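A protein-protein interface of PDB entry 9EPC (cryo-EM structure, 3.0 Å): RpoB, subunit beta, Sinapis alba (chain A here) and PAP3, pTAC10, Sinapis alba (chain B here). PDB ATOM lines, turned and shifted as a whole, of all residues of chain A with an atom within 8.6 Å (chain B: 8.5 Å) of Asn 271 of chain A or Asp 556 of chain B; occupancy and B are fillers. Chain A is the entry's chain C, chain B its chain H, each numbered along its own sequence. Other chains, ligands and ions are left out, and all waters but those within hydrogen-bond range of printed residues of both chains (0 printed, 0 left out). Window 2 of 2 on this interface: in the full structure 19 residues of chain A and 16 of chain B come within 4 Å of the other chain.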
ATOM      1  N   ILE A 132      21.333  22.650   8.271  1.00  0.00           N
ATOM      2  CA  ILE A 132      20.100  23.238   7.761  1.00  0.00           C
ATOM      3  C   ILE A 132      18.914  22.521   8.388  1.00  0.00           C
ATOM      4  O   ILE A 132      18.908  21.292   8.519  1.00  0.00           O
ATOM      5  CB  ILE A 132      20.054  23.162   6.223  1.00  0.00           C
ATOM      6  CG1 ILE A 132      18.708  23.662   5.695  1.00  0.00           C
ATOM      7  CG2 ILE A 132      20.325  21.745   5.746  1.00  0.00           C
ATOM      8  CD1 ILE A 132      18.413  25.104   6.035  1.00  0.00           C
ATOM      9  N   ILE A 194      24.052  30.700 -12.155  1.00  0.00           N
ATOM     10  CA  ILE A 194      23.615  29.377 -11.721  1.00  0.00           C
ATOM     11  C   ILE A 194      22.238  29.401 -11.078  1.00  0.00           C
ATOM     12  O   ILE A 194      21.671  28.326 -10.824  1.00  0.00           O
ATOM     13  CB  ILE A 194      24.637  28.734 -10.758  1.00  0.00           C
ATOM     14  CG1 ILE A 194      26.060  29.154 -11.128  1.00  0.00           C
ATOM     15  CG2 ILE A 194      24.537  27.215 -10.797  1.00  0.00           C
ATOM     16  CD1 ILE A 194      26.550  28.578 -12.442  1.00  0.00           C
ATOM     17  N   ASN A 197      19.824  27.519 -13.220  1.00  0.00           N
ATOM     18  CA  ASN A 197      20.161  26.152 -13.589  1.00  0.00           C
ATOM     19  C   ASN A 197      19.363  25.109 -12.817  1.00  0.00           C
ATOM     20  O   ASN A 197      19.471  23.918 -13.130  1.00  0.00           O
ATOM     21  CB  ASN A 197      21.658  25.901 -13.388  1.00  0.00           C
ATOM     22  CG  ASN A 197      22.508  26.594 -14.433  1.00  0.00           C
ATOM     23  OD1 ASN A 197      23.500  27.247 -14.110  1.00  0.00           O
ATOM     24  ND2 ASN A 197      22.122  26.457 -15.695  1.00  0.00           N
ATOM     25  N   VAL A 198      18.578  25.516 -11.824  1.00  0.00           N
ATOM     26  CA  VAL A 198      17.755  24.595 -11.045  1.00  0.00           C
ATOM     27  C   VAL A 198      16.375  25.211 -10.853  1.00  0.00           C
ATOM     28  O   VAL A 198      16.259  26.372 -10.445  1.00  0.00           O
ATOM     29  CB  VAL A 198      18.403  24.256  -9.687  1.00  0.00           C
ATOM     30  CG1 VAL A 198      18.872  25.522  -8.981  1.00  0.00           C
ATOM     31  CG2 VAL A 198      17.434  23.475  -8.815  1.00  0.00           C
ATOM     32  N   ARG A 263      29.353  20.867   7.766  1.00  0.00           N
ATOM     33  CA  ARG A 263      29.549  20.492   6.370  1.00  0.00           C
ATOM     34  C   ARG A 263      28.950  19.123   6.079  1.00  0.00           C
ATOM     35  O   ARG A 263      28.365  18.906   5.011  1.00  0.00           O
ATOM     36  CB  ARG A 263      31.037  20.516   6.023  1.00  0.00           C
ATOM     37  CG  ARG A 263      31.349  20.106   4.591  1.00  0.00           C
ATOM     38  CD  ARG A 263      30.522  20.898   3.591  1.00  0.00           C
ATOM     39  NE  ARG A 263      30.748  22.333   3.704  1.00  0.00           N
ATOM     40  CZ  ARG A 263      30.049  23.252   3.055  1.00  0.00           C
ATOM     41  NH1 ARG A 263      29.060  22.921   2.241  1.00  0.00           N
ATOM     42  NH2 ARG A 263      30.347  24.537   3.230  1.00  0.00           N
ATOM     43  N   ARG A 264      29.095  18.181   7.011  1.00  0.00           N
ATOM     44  CA  ARG A 264      28.493  16.865   6.827  1.00  0.00           C
ATOM     45  C   ARG A 264      26.974  16.960   6.774  1.00  0.00           C
ATOM     46  O   ARG A 264      26.331  16.340   5.920  1.00  0.00           O
ATOM     47  CB  ARG A 264      28.940  15.928   7.948  1.00  0.00           C
ATOM     48  CG  ARG A 264      28.098  14.672   8.082  1.00  0.00           C
ATOM     49  CD  ARG A 264      28.663  13.752   9.147  1.00  0.00           C
ATOM     50  NE  ARG A 264      27.689  12.760   9.585  1.00  0.00           N
ATOM     51  CZ  ARG A 264      26.850  12.937  10.597  1.00  0.00           C
ATOM     52  NH1 ARG A 264      26.841  14.058  11.299  1.00  0.00           N
ATOM     53  NH2 ARG A 264      26.000  11.964  10.913  1.00  0.00           N
ATOM     54  N   ASN A 265      26.380  17.748   7.673  1.00  0.00           N
ATOM     55  CA  ASN A 265      24.925  17.831   7.730  1.00  0.00           C
ATOM     56  C   ASN A 265      24.360  18.611   6.551  1.00  0.00           C
ATOM     57  O   ASN A 265      23.306  18.252   6.013  1.00  0.00           O
ATOM     58  CB  ASN A 265      24.485  18.458   9.051  1.00  0.00           C
ATOM     59  CG  ASN A 265      24.722  17.545  10.234  1.00  0.00           C
ATOM     60  OD1 ASN A 265      25.586  16.670  10.193  1.00  0.00           O
ATOM     61  ND2 ASN A 265      23.951  17.741  11.296  1.00  0.00           N
ATOM     62  N   ILE A 266      25.036  19.685   6.137  1.00  0.00           N
ATOM     63  CA  ILE A 266      24.536  20.467   5.012  1.00  0.00           C
ATOM     64  C   ILE A 266      24.590  19.651   3.727  1.00  0.00           C
ATOM     65  O   ILE A 266      23.716  19.783   2.863  1.00  0.00           O
ATOM     66  CB  ILE A 266      25.306  21.797   4.887  1.00  0.00           C
ATOM     67  CG1 ILE A 266      24.578  22.752   3.942  1.00  0.00           C
ATOM     68  CG2 ILE A 266      26.723  21.576   4.401  1.00  0.00           C
ATOM     69  CD1 ILE A 266      23.342  23.365   4.542  1.00  0.00           C
ATOM     70  N   ASN A 267      25.602  18.793   3.577  1.00  0.00           N
ATOM     71  CA  ASN A 267      25.650  17.890   2.435  1.00  0.00           C
ATOM     72  C   ASN A 267      24.684  16.726   2.594  1.00  0.00           C
ATOM     73  O   ASN A 267      24.146  16.235   1.597  1.00  0.00           O
ATOM     74  CB  ASN A 267      27.068  17.357   2.238  1.00  0.00           C
ATOM     75  CG  ASN A 267      28.059  18.449   1.904  1.00  0.00           C
ATOM     76  OD1 ASN A 267      27.778  19.633   2.081  1.00  0.00           O
ATOM     77  ND2 ASN A 267      29.231  18.056   1.421  1.00  0.00           N
ATOM     78  N   TRP A 268      24.461  16.271   3.828  1.00  0.00           N
ATOM     79  CA  TRP A 268      23.591  15.122   4.049  1.00  0.00           C
ATOM     80  C   TRP A 268      22.164  15.413   3.606  1.00  0.00           C
ATOM     81  O   TRP A 268      21.515  14.565   2.984  1.00  0.00           O
ATOM     82  CB  TRP A 268      23.620  14.723   5.524  1.00  0.00           C
ATOM     83  CG  TRP A 268      22.960  13.416   5.809  1.00  0.00           C
ATOM     84  CD1 TRP A 268      21.620  13.164   5.852  1.00  0.00           C
ATOM     85  CD2 TRP A 268      23.610  12.176   6.107  1.00  0.00           C
ATOM     86  NE1 TRP A 268      21.396  11.843   6.151  1.00  0.00           N
ATOM     87  CE2 TRP A 268      22.602  11.215   6.314  1.00  0.00           C
ATOM     88  CE3 TRP A 268      24.948  11.785   6.218  1.00  0.00           C
ATOM     89  CZ2 TRP A 268      22.888   9.887   6.624  1.00  0.00           C
ATOM     90  CZ3 TRP A 268      25.231  10.467   6.525  1.00  0.00           C
ATOM     91  CH2 TRP A 268      24.206   9.534   6.724  1.00  0.00           C
ATOM     92  N   ARG A 269      21.659  16.604   3.918  1.00  0.00           N
ATOM     93  CA  ARG A 269      20.282  16.950   3.594  1.00  0.00           C
ATOM     94  C   ARG A 269      20.138  17.494   2.177  1.00  0.00           C
ATOM     95  O   ARG A 269      19.233  17.087   1.443  1.00  0.00           O
ATOM     96  CB  ARG A 269      19.743  17.962   4.608  1.00  0.00           C
ATOM     97  CG  ARG A 269      18.520  18.717   4.129  1.00  0.00           C
ATOM     98  CD  ARG A 269      17.677  19.194   5.293  1.00  0.00           C
ATOM     99  NE  ARG A 269      16.995  18.085   5.949  1.00  0.00           N
ATOM    100  CZ  ARG A 269      15.820  17.602   5.569  1.00  0.00           C
ATOM    101  NH1 ARG A 269      15.166  18.109   4.537  1.00  0.00           N
ATOM    102  NH2 ARG A 269      15.288  16.586   6.241  1.00  0.00           N
ATOM    103  N   LEU A 270      21.018  18.408   1.777  1.00  0.00           N
ATOM    104  CA  LEU A 270      20.911  19.045   0.472  1.00  0.00           C
ATOM    105  C   LEU A 270      21.559  18.241  -0.646  1.00  0.00           C
ATOM    106  O   LEU A 270      21.434  18.631  -1.813  1.00  0.00           O
ATOM    107  CB  LEU A 270      21.529  20.444   0.517  1.00  0.00           C
ATOM    108  CG  LEU A 270      20.920  21.401   1.543  1.00  0.00           C
ATOM    109  CD1 LEU A 270      21.512  22.791   1.396  1.00  0.00           C
ATOM    110  CD2 LEU A 270      19.407  21.442   1.405  1.00  0.00           C
ATOM    111  N   ASN A 271      22.232  17.138  -0.326  1.00  0.00           N
ATOM    112  CA  ASN A 271      22.894  16.287  -1.314  1.00  0.00           C
ATOM    113  C   ASN A 271      23.841  17.102  -2.194  1.00  0.00           C
ATOM    114  O   ASN A 271      23.662  17.231  -3.406  1.00  0.00           O
ATOM    115  CB  ASN A 271      21.868  15.527  -2.156  1.00  0.00           C
ATOM    116  CG  ASN A 271      21.184  14.423  -1.378  1.00  0.00           C
ATOM    117  OD1 ASN A 271      21.193  14.419  -0.148  1.00  0.00           O
ATOM    118  ND2 ASN A 271      20.588  13.476  -2.093  1.00  0.00           N
ATOM    119  N   LEU A 272      24.859  17.663  -1.551  1.00  0.00           N
ATOM    120  CA  LEU A 272      25.845  18.499  -2.216  1.00  0.00           C
ATOM    121  C   LEU A 272      27.158  17.743  -2.358  1.00  0.00           C
ATOM    122  O   LEU A 272      27.528  16.948  -1.488  1.00  0.00           O
ATOM    123  CB  LEU A 272      26.068  19.801  -1.445  1.00  0.00           C
ATOM    124  CG  LEU A 272      24.812  20.638  -1.202  1.00  0.00           C
ATOM    125  CD1 LEU A 272      25.166  21.966  -0.555  1.00  0.00           C
ATOM    126  CD2 LEU A 272      24.053  20.854  -2.500  1.00  0.00           C
ATOM    127  N   ASN A 273      27.857  17.996  -3.461  1.00  0.00           N
ATOM    128  CA  ASN A 273      29.109  17.320  -3.773  1.00  0.00           C
ATOM    129  C   ASN A 273      30.323  18.016  -3.172  1.00  0.00           C
ATOM    130  O   ASN A 273      31.452  17.569  -3.400  1.00  0.00           O
ATOM    131  CB  ASN A 273      29.272  17.207  -5.294  1.00  0.00           C
ATOM    132  CG  ASN A 273      30.251  16.124  -5.698  1.00  0.00           C
ATOM    133  OD1 ASN A 273      31.415  16.398  -5.988  1.00  0.00           O
ATOM    134  ND2 ASN A 273      29.783  14.881  -5.719  1.00  0.00           N
ATOM    135  N   ILE A 274      30.121  19.090  -2.415  1.00  0.00           N
ATOM    136  CA  ILE A 274      31.250  19.805  -1.809  1.00  0.00           C
ATOM    137  C   ILE A 274      31.967  18.880  -0.832  1.00  0.00           C
ATOM    138  O   ILE A 274      31.317  18.289   0.053  1.00  0.00           O
ATOM    139  CB  ILE A 274      30.760  21.084  -1.106  1.00  0.00           C
ATOM    140  CG1 ILE A 274      31.792  21.582  -0.093  1.00  0.00           C
ATOM    141  CG2 ILE A 274      29.413  20.850  -0.448  1.00  0.00           C
ATOM    142  CD1 ILE A 274      32.983  22.259  -0.721  1.00  0.00           C
ATOM    143  N   ARG A 284      26.661  28.110  -3.122  1.00  0.00           N
ATOM    144  CA  ARG A 284      25.963  26.919  -3.589  1.00  0.00           C
ATOM    145  C   ARG A 284      25.081  26.342  -2.492  1.00  0.00           C
ATOM    146  O   ARG A 284      23.943  25.931  -2.749  1.00  0.00           O
ATOM    147  CB  ARG A 284      26.976  25.881  -4.070  1.00  0.00           C
ATOM    148  CG  ARG A 284      26.436  24.466  -4.149  1.00  0.00           C
ATOM    149  CD  ARG A 284      25.413  24.317  -5.257  1.00  0.00           C
ATOM    150  NE  ARG A 284      24.834  22.980  -5.272  1.00  0.00           N
ATOM    151  CZ  ARG A 284      25.409  21.921  -5.826  1.00  0.00           C
ATOM    152  NH1 ARG A 284      26.586  22.009  -6.424  1.00  0.00           N
ATOM    153  NH2 ARG A 284      24.788  20.746  -5.778  1.00  0.00           N
ATOM    154  N   ASP A 285      25.590  26.307  -1.259  1.00  0.00           N
ATOM    155  CA  ASP A 285      24.787  25.827  -0.140  1.00  0.00           C
ATOM    156  C   ASP A 285      23.570  26.714   0.082  1.00  0.00           C
ATOM    157  O   ASP A 285      22.465  26.216   0.324  1.00  0.00           O
ATOM    158  CB  ASP A 285      25.643  25.763   1.125  1.00  0.00           C
ATOM    159  CG  ASP A 285      27.039  25.236   0.858  1.00  0.00           C
ATOM    160  OD1 ASP A 285      27.208  24.462  -0.107  1.00  0.00           O
ATOM    161  OD2 ASP A 285      27.967  25.600   1.609  1.00  0.00           O
ATOM    162  N   ALA A 288      21.228  25.978  -2.756  1.00  0.00           N
ATOM    163  CA  ALA A 288      20.547  24.709  -2.539  1.00  0.00           C
ATOM    164  C   ALA A 288      19.551  24.774  -1.389  1.00  0.00           C
ATOM    165  O   ALA A 288      18.638  23.945  -1.332  1.00  0.00           O
ATOM    166  CB  ALA A 288      21.567  23.600  -2.282  1.00  0.00           C
ATOM    167  N   ASP A 291      16.399  25.542  -2.889  1.00  0.00           N
ATOM    168  CA  ASP A 291      15.999  24.470  -3.793  1.00  0.00           C
ATOM    169  C   ASP A 291      15.127  23.444  -3.078  1.00  0.00           C
ATOM    170  O   ASP A 291      14.031  23.111  -3.543  1.00  0.00           O
ATOM    171  CB  ASP A 291      17.239  23.803  -4.389  1.00  0.00           C
ATOM    172  CG  ASP A 291      16.899  22.789  -5.462  1.00  0.00           C
ATOM    173  OD1 ASP A 291      15.744  22.780  -5.934  1.00  0.00           O
ATOM    174  OD2 ASP A 291      17.790  21.998  -5.834  1.00  0.00           O
ATOM    175  N   HIS A 292      15.599  22.931  -1.941  1.00  0.00           N
ATOM    176  CA  HIS A 292      14.788  22.003  -1.161  1.00  0.00           C
ATOM    177  C   HIS A 292      13.652  22.706  -0.435  1.00  0.00           C
ATOM    178  O   HIS A 292      12.667  22.055  -0.072  1.00  0.00           O
ATOM    179  CB  HIS A 292      15.662  21.250  -0.159  1.00  0.00           C
ATOM    180  CG  HIS A 292      16.500  20.176  -0.777  1.00  0.00           C
ATOM    181  ND1 HIS A 292      16.138  18.846  -0.756  1.00  0.00           N
ATOM    182  CD2 HIS A 292      17.682  20.234  -1.436  1.00  0.00           C
ATOM    183  CE1 HIS A 292      17.061  18.132  -1.374  1.00  0.00           C
ATOM    184  NE2 HIS A 292      18.009  18.949  -1.796  1.00  0.00           N
ATOM    185  N   LYS B 386      35.658  13.327 -19.458  1.00  0.00           N
ATOM    186  CA  LYS B 386      35.591  14.772 -19.618  1.00  0.00           C
ATOM    187  C   LYS B 386      36.661  15.230 -20.598  1.00  0.00           C
ATOM    188  O   LYS B 386      37.830  14.849 -20.481  1.00  0.00           O
ATOM    189  CB  LYS B 386      35.771  15.463 -18.268  1.00  0.00           C
ATOM    190  CG  LYS B 386      34.740  15.057 -17.228  1.00  0.00           C
ATOM    191  CD  LYS B 386      34.972  15.764 -15.905  1.00  0.00           C
ATOM    192  CE  LYS B 386      33.960  15.322 -14.862  1.00  0.00           C
ATOM    193  NZ  LYS B 386      34.180  15.996 -13.552  1.00  0.00           N
ATOM    194  N   SER B 551      29.209  18.970 -18.925  1.00  0.00           N
ATOM    195  CA  SER B 551      27.908  18.883 -18.268  1.00  0.00           C
ATOM    196  C   SER B 551      27.227  17.540 -18.496  1.00  0.00           C
ATOM    197  O   SER B 551      26.131  17.321 -17.966  1.00  0.00           O
ATOM    198  CB  SER B 551      26.949  20.003 -18.699  1.00  0.00           C
ATOM    199  OG  SER B 551      26.558  19.849 -20.052  1.00  0.00           O
ATOM    200  N   PHE B 553      28.422  14.711 -17.367  1.00  0.00           N
ATOM    201  CA  PHE B 553      28.673  13.932 -16.155  1.00  0.00           C
ATOM    202  C   PHE B 553      27.939  14.587 -14.989  1.00  0.00           C
ATOM    203  O   PHE B 553      28.514  15.302 -14.165  1.00  0.00           O
ATOM    204  CB  PHE B 553      30.170  13.821 -15.897  1.00  0.00           C
ATOM    205  CG  PHE B 553      30.933  13.224 -17.041  1.00  0.00           C
ATOM    206  CD1 PHE B 553      31.426  14.027 -18.055  1.00  0.00           C
ATOM    207  CD2 PHE B 553      31.154  11.860 -17.105  1.00  0.00           C
ATOM    208  CE1 PHE B 553      32.127  13.480 -19.110  1.00  0.00           C
ATOM    209  CE2 PHE B 553      31.855  11.308 -18.157  1.00  0.00           C
ATOM    210  CZ  PHE B 553      32.340  12.119 -19.161  1.00  0.00           C
ATOM    211  N   GLY B 554      26.637  14.333 -14.929  1.00  0.00           N
ATOM    212  CA  GLY B 554      25.829  14.847 -13.846  1.00  0.00           C
ATOM    213  C   GLY B 554      25.597  16.345 -13.955  1.00  0.00           C
ATOM    214  O   GLY B 554      25.882  16.990 -14.966  1.00  0.00           O
ATOM    215  N   LYS B 555      25.063  16.898 -12.865  1.00  0.00           N
ATOM    216  CA  LYS B 555      24.778  18.322 -12.778  1.00  0.00           C
ATOM    217  C   LYS B 555      25.537  19.034 -11.670  1.00  0.00           C
ATOM    218  O   LYS B 555      25.687  20.258 -11.742  1.00  0.00           O
ATOM    219  CB  LYS B 555      23.273  18.557 -12.572  1.00  0.00           C
ATOM    220  CG  LYS B 555      22.390  17.763 -13.520  1.00  0.00           C
ATOM    221  CD  LYS B 555      22.744  18.042 -14.970  1.00  0.00           C
ATOM    222  CE  LYS B 555      21.980  17.124 -15.909  1.00  0.00           C
ATOM    223  NZ  LYS B 555      22.390  17.319 -17.327  1.00  0.00           N
ATOM    224  N   ASP B 556      26.015  18.315 -10.658  1.00  0.00           N
ATOM    225  CA  ASP B 556      26.747  18.898  -9.537  1.00  0.00           C
ATOM    226  C   ASP B 556      28.218  18.523  -9.682  1.00  0.00           C
ATOM    227  O   ASP B 556      28.606  17.383  -9.414  1.00  0.00           O
ATOM    228  CB  ASP B 556      26.180  18.411  -8.206  1.00  0.00           C
ATOM    229  CG  ASP B 556      24.694  18.669  -8.075  1.00  0.00           C
ATOM    230  OD1 ASP B 556      24.101  19.242  -9.012  1.00  0.00           O
ATOM    231  OD2 ASP B 556      24.117  18.299  -7.031  1.00  0.00           O
ATOM    232  N   GLN B 557      29.033  19.486 -10.105  1.00  0.00           N
ATOM    233  CA  GLN B 557      30.473  19.302 -10.232  1.00  0.00           C
ATOM    234  C   GLN B 557      31.171  20.353  -9.384  1.00  0.00           C
ATOM    235  O   GLN B 557      30.926  21.553  -9.554  1.00  0.00           O
ATOM    236  CB  GLN B 557      30.923  19.405 -11.692  1.00  0.00           C
ATOM    237  CG  GLN B 557      30.383  18.311 -12.602  1.00  0.00           C
ATOM    238  CD  GLN B 557      28.962  18.572 -13.061  1.00  0.00           C
ATOM    239  OE1 GLN B 557      28.360  19.585 -12.707  1.00  0.00           O
ATOM    240  NE2 GLN B 557      28.421  17.659 -13.858  1.00  0.00           N
ATOM    241  N   TYR B 558      32.035  19.906  -8.477  1.00  0.00           N
ATOM    242  CA  TYR B 558      32.769  20.821  -7.611  1.00  0.00           C
ATOM    243  C   TYR B 558      33.797  21.584  -8.436  1.00  0.00           C
ATOM    244  O   TYR B 558      34.804  21.016  -8.869  1.00  0.00           O
ATOM    245  CB  TYR B 558      33.439  20.053  -6.476  1.00  0.00           C
ATOM    246  CG  TYR B 558      34.334  20.908  -5.611  1.00  0.00           C
ATOM    247  CD1 TYR B 558      33.799  21.789  -4.682  1.00  0.00           C
ATOM    248  CD2 TYR B 558      35.716  20.834  -5.723  1.00  0.00           C
ATOM    249  CE1 TYR B 558      34.613  22.573  -3.890  1.00  0.00           C
ATOM    250  CE2 TYR B 558      36.539  21.613  -4.935  1.00  0.00           C
ATOM    251  CZ  TYR B 558      35.983  22.481  -4.020  1.00  0.00           C
ATOM    252  OH  TYR B 558      36.797  23.260  -3.232  1.00  0.00           O
ATOM    253  N   ASP B 559      33.547  22.875  -8.653  1.00  0.00           N
ATOM    254  CA  ASP B 559      34.429  23.742  -9.432  1.00  0.00           C
ATOM    255  C   ASP B 559      34.904  24.872  -8.529  1.00  0.00           C
ATOM    256  O   ASP B 559      34.231  25.906  -8.405  1.00  0.00           O
ATOM    257  CB  ASP B 559      33.717  24.286 -10.667  1.00  0.00           C
ATOM    258  CG  ASP B 559      34.639  25.078 -11.573  1.00  0.00           C
ATOM    259  OD1 ASP B 559      35.869  25.039 -11.357  1.00  0.00           O
ATOM    260  OD2 ASP B 559      34.135  25.742 -12.502  1.00  0.00           O
ATOM    261  N   LEU B 564      30.591  29.922  -7.703  1.00  0.00           N
ATOM    262  CA  LEU B 564      29.602  29.148  -6.960  1.00  0.00           C
ATOM    263  C   LEU B 564      30.243  28.424  -5.784  1.00  0.00           C
ATOM    264  O   LEU B 564      29.643  28.319  -4.708  1.00  0.00           O
ATOM    265  CB  LEU B 564      28.911  28.153  -7.892  1.00  0.00           C
ATOM    266  CG  LEU B 564      27.722  27.393  -7.306  1.00  0.00           C
ATOM    267  CD1 LEU B 564      26.607  28.357  -6.935  1.00  0.00           C
ATOM    268  CD2 LEU B 564      27.225  26.338  -8.280  1.00  0.00           C
ATOM    269  N   TYR B 565      31.456  27.910  -5.972  1.00  0.00           N
ATOM    270  CA  TYR B 565      32.179  27.209  -4.922  1.00  0.00           C
ATOM    271  C   TYR B 565      33.280  28.051  -4.293  1.00  0.00           C
ATOM    272  O   TYR B 565      34.004  27.550  -3.428  1.00  0.00           O
ATOM    273  CB  TYR B 565      32.776  25.909  -5.472  1.00  0.00           C
ATOM    274  CG  TYR B 565      31.753  24.963  -6.060  1.00  0.00           C
ATOM    275  CD1 TYR B 565      31.367  25.065  -7.389  1.00  0.00           C
ATOM    276  CD2 TYR B 565      31.177  23.965  -5.285  1.00  0.00           C
ATOM    277  CE1 TYR B 565      30.433  24.202  -7.931  1.00  0.00           C
ATOM    278  CE2 TYR B 565      30.244  23.097  -5.818  1.00  0.00           C
ATOM    279  CZ  TYR B 565      29.875  23.220  -7.140  1.00  0.00           C
ATOM    280  OH  TYR B 565      28.947  22.358  -7.676  1.00  0.00           O
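Ile 194 of chain A touches Leu 564 of chain B (CG2 to CD2, 3.8 Å).
OD2 of Asp 556 of chain B touches O of Asn 271 of chain A, at 3.8 Å.
Ile 274 of chain A touches Tyr 558 of chain B.
OH of Tyr 565 of chain B sits at hydrogen-bond distance from NH1 of Arg 284 of chain A (2.7 Å).
The guanidinium group (NH2) of Arg 284 of chain A is in salt-bridge range of the side-chain carboxylate (OD2) of Asp 556 of chain B (2.8 Å).
N of Arg 284 of chain A is in hydrogen-bond range of O of Leu 564 of chain B, at 3.4 Å.
Hydrophobic or aromatic side chains of chain B within 4 Å of the printed part of chain A: Tyr 558, Leu 564 and Tyr 565.
Among the printed residues, Asp or Glu carboxylates within 4 Å of a Lys or Arg side-chain nitrogen of the other chain: Arg 284 of chain A with Asp 556 of chain B.
O of Gln 557 of chain B sits at hydrogen-bond distance from OH of Tyr 565 of chain B (2.8 Å).
The backbone carbonyl oxygen (O) of Ile 274 of chain A lies within hydrogen-bond range of the side-chain amide nitrogen (ND2) of Asn 267 of chain A (2.5 Å).
The backbone carbonyl oxygen (O) of Trp 268 of chain A sits close to the side-chain amide oxygen (OD1) of Asn 271 of chain A (3.2 Å).
Of chain B, only Asp 556 (3.8 Å) comes within 4 Å of Asn 271 of chain A.
Asp 556 of chain B touches just these residues of chain A: Asn 271 (3.8 Å) and Arg 284 (2.8 Å).
No residue of chain A comes within 4 Å of Gln 557 of chain B.
Printed residues of chain B within 4 Å of Ile 274 of chain A: Tyr 558 (3.6 Å).
Of the printed residues of chain A, Leu 564 of chain B touches Ile 194 and Arg 284.
Of the printed residues of chain B, Arg 284 of chain A touches Asp 556, Leu 564 and Tyr 565.
Ile 266 of chain A touches none of the printed residues of chain B.
The nearest printed residue of chain B that does not touch Asn 271 of chain A is Tyr 565 of chain B (8.5 Å).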
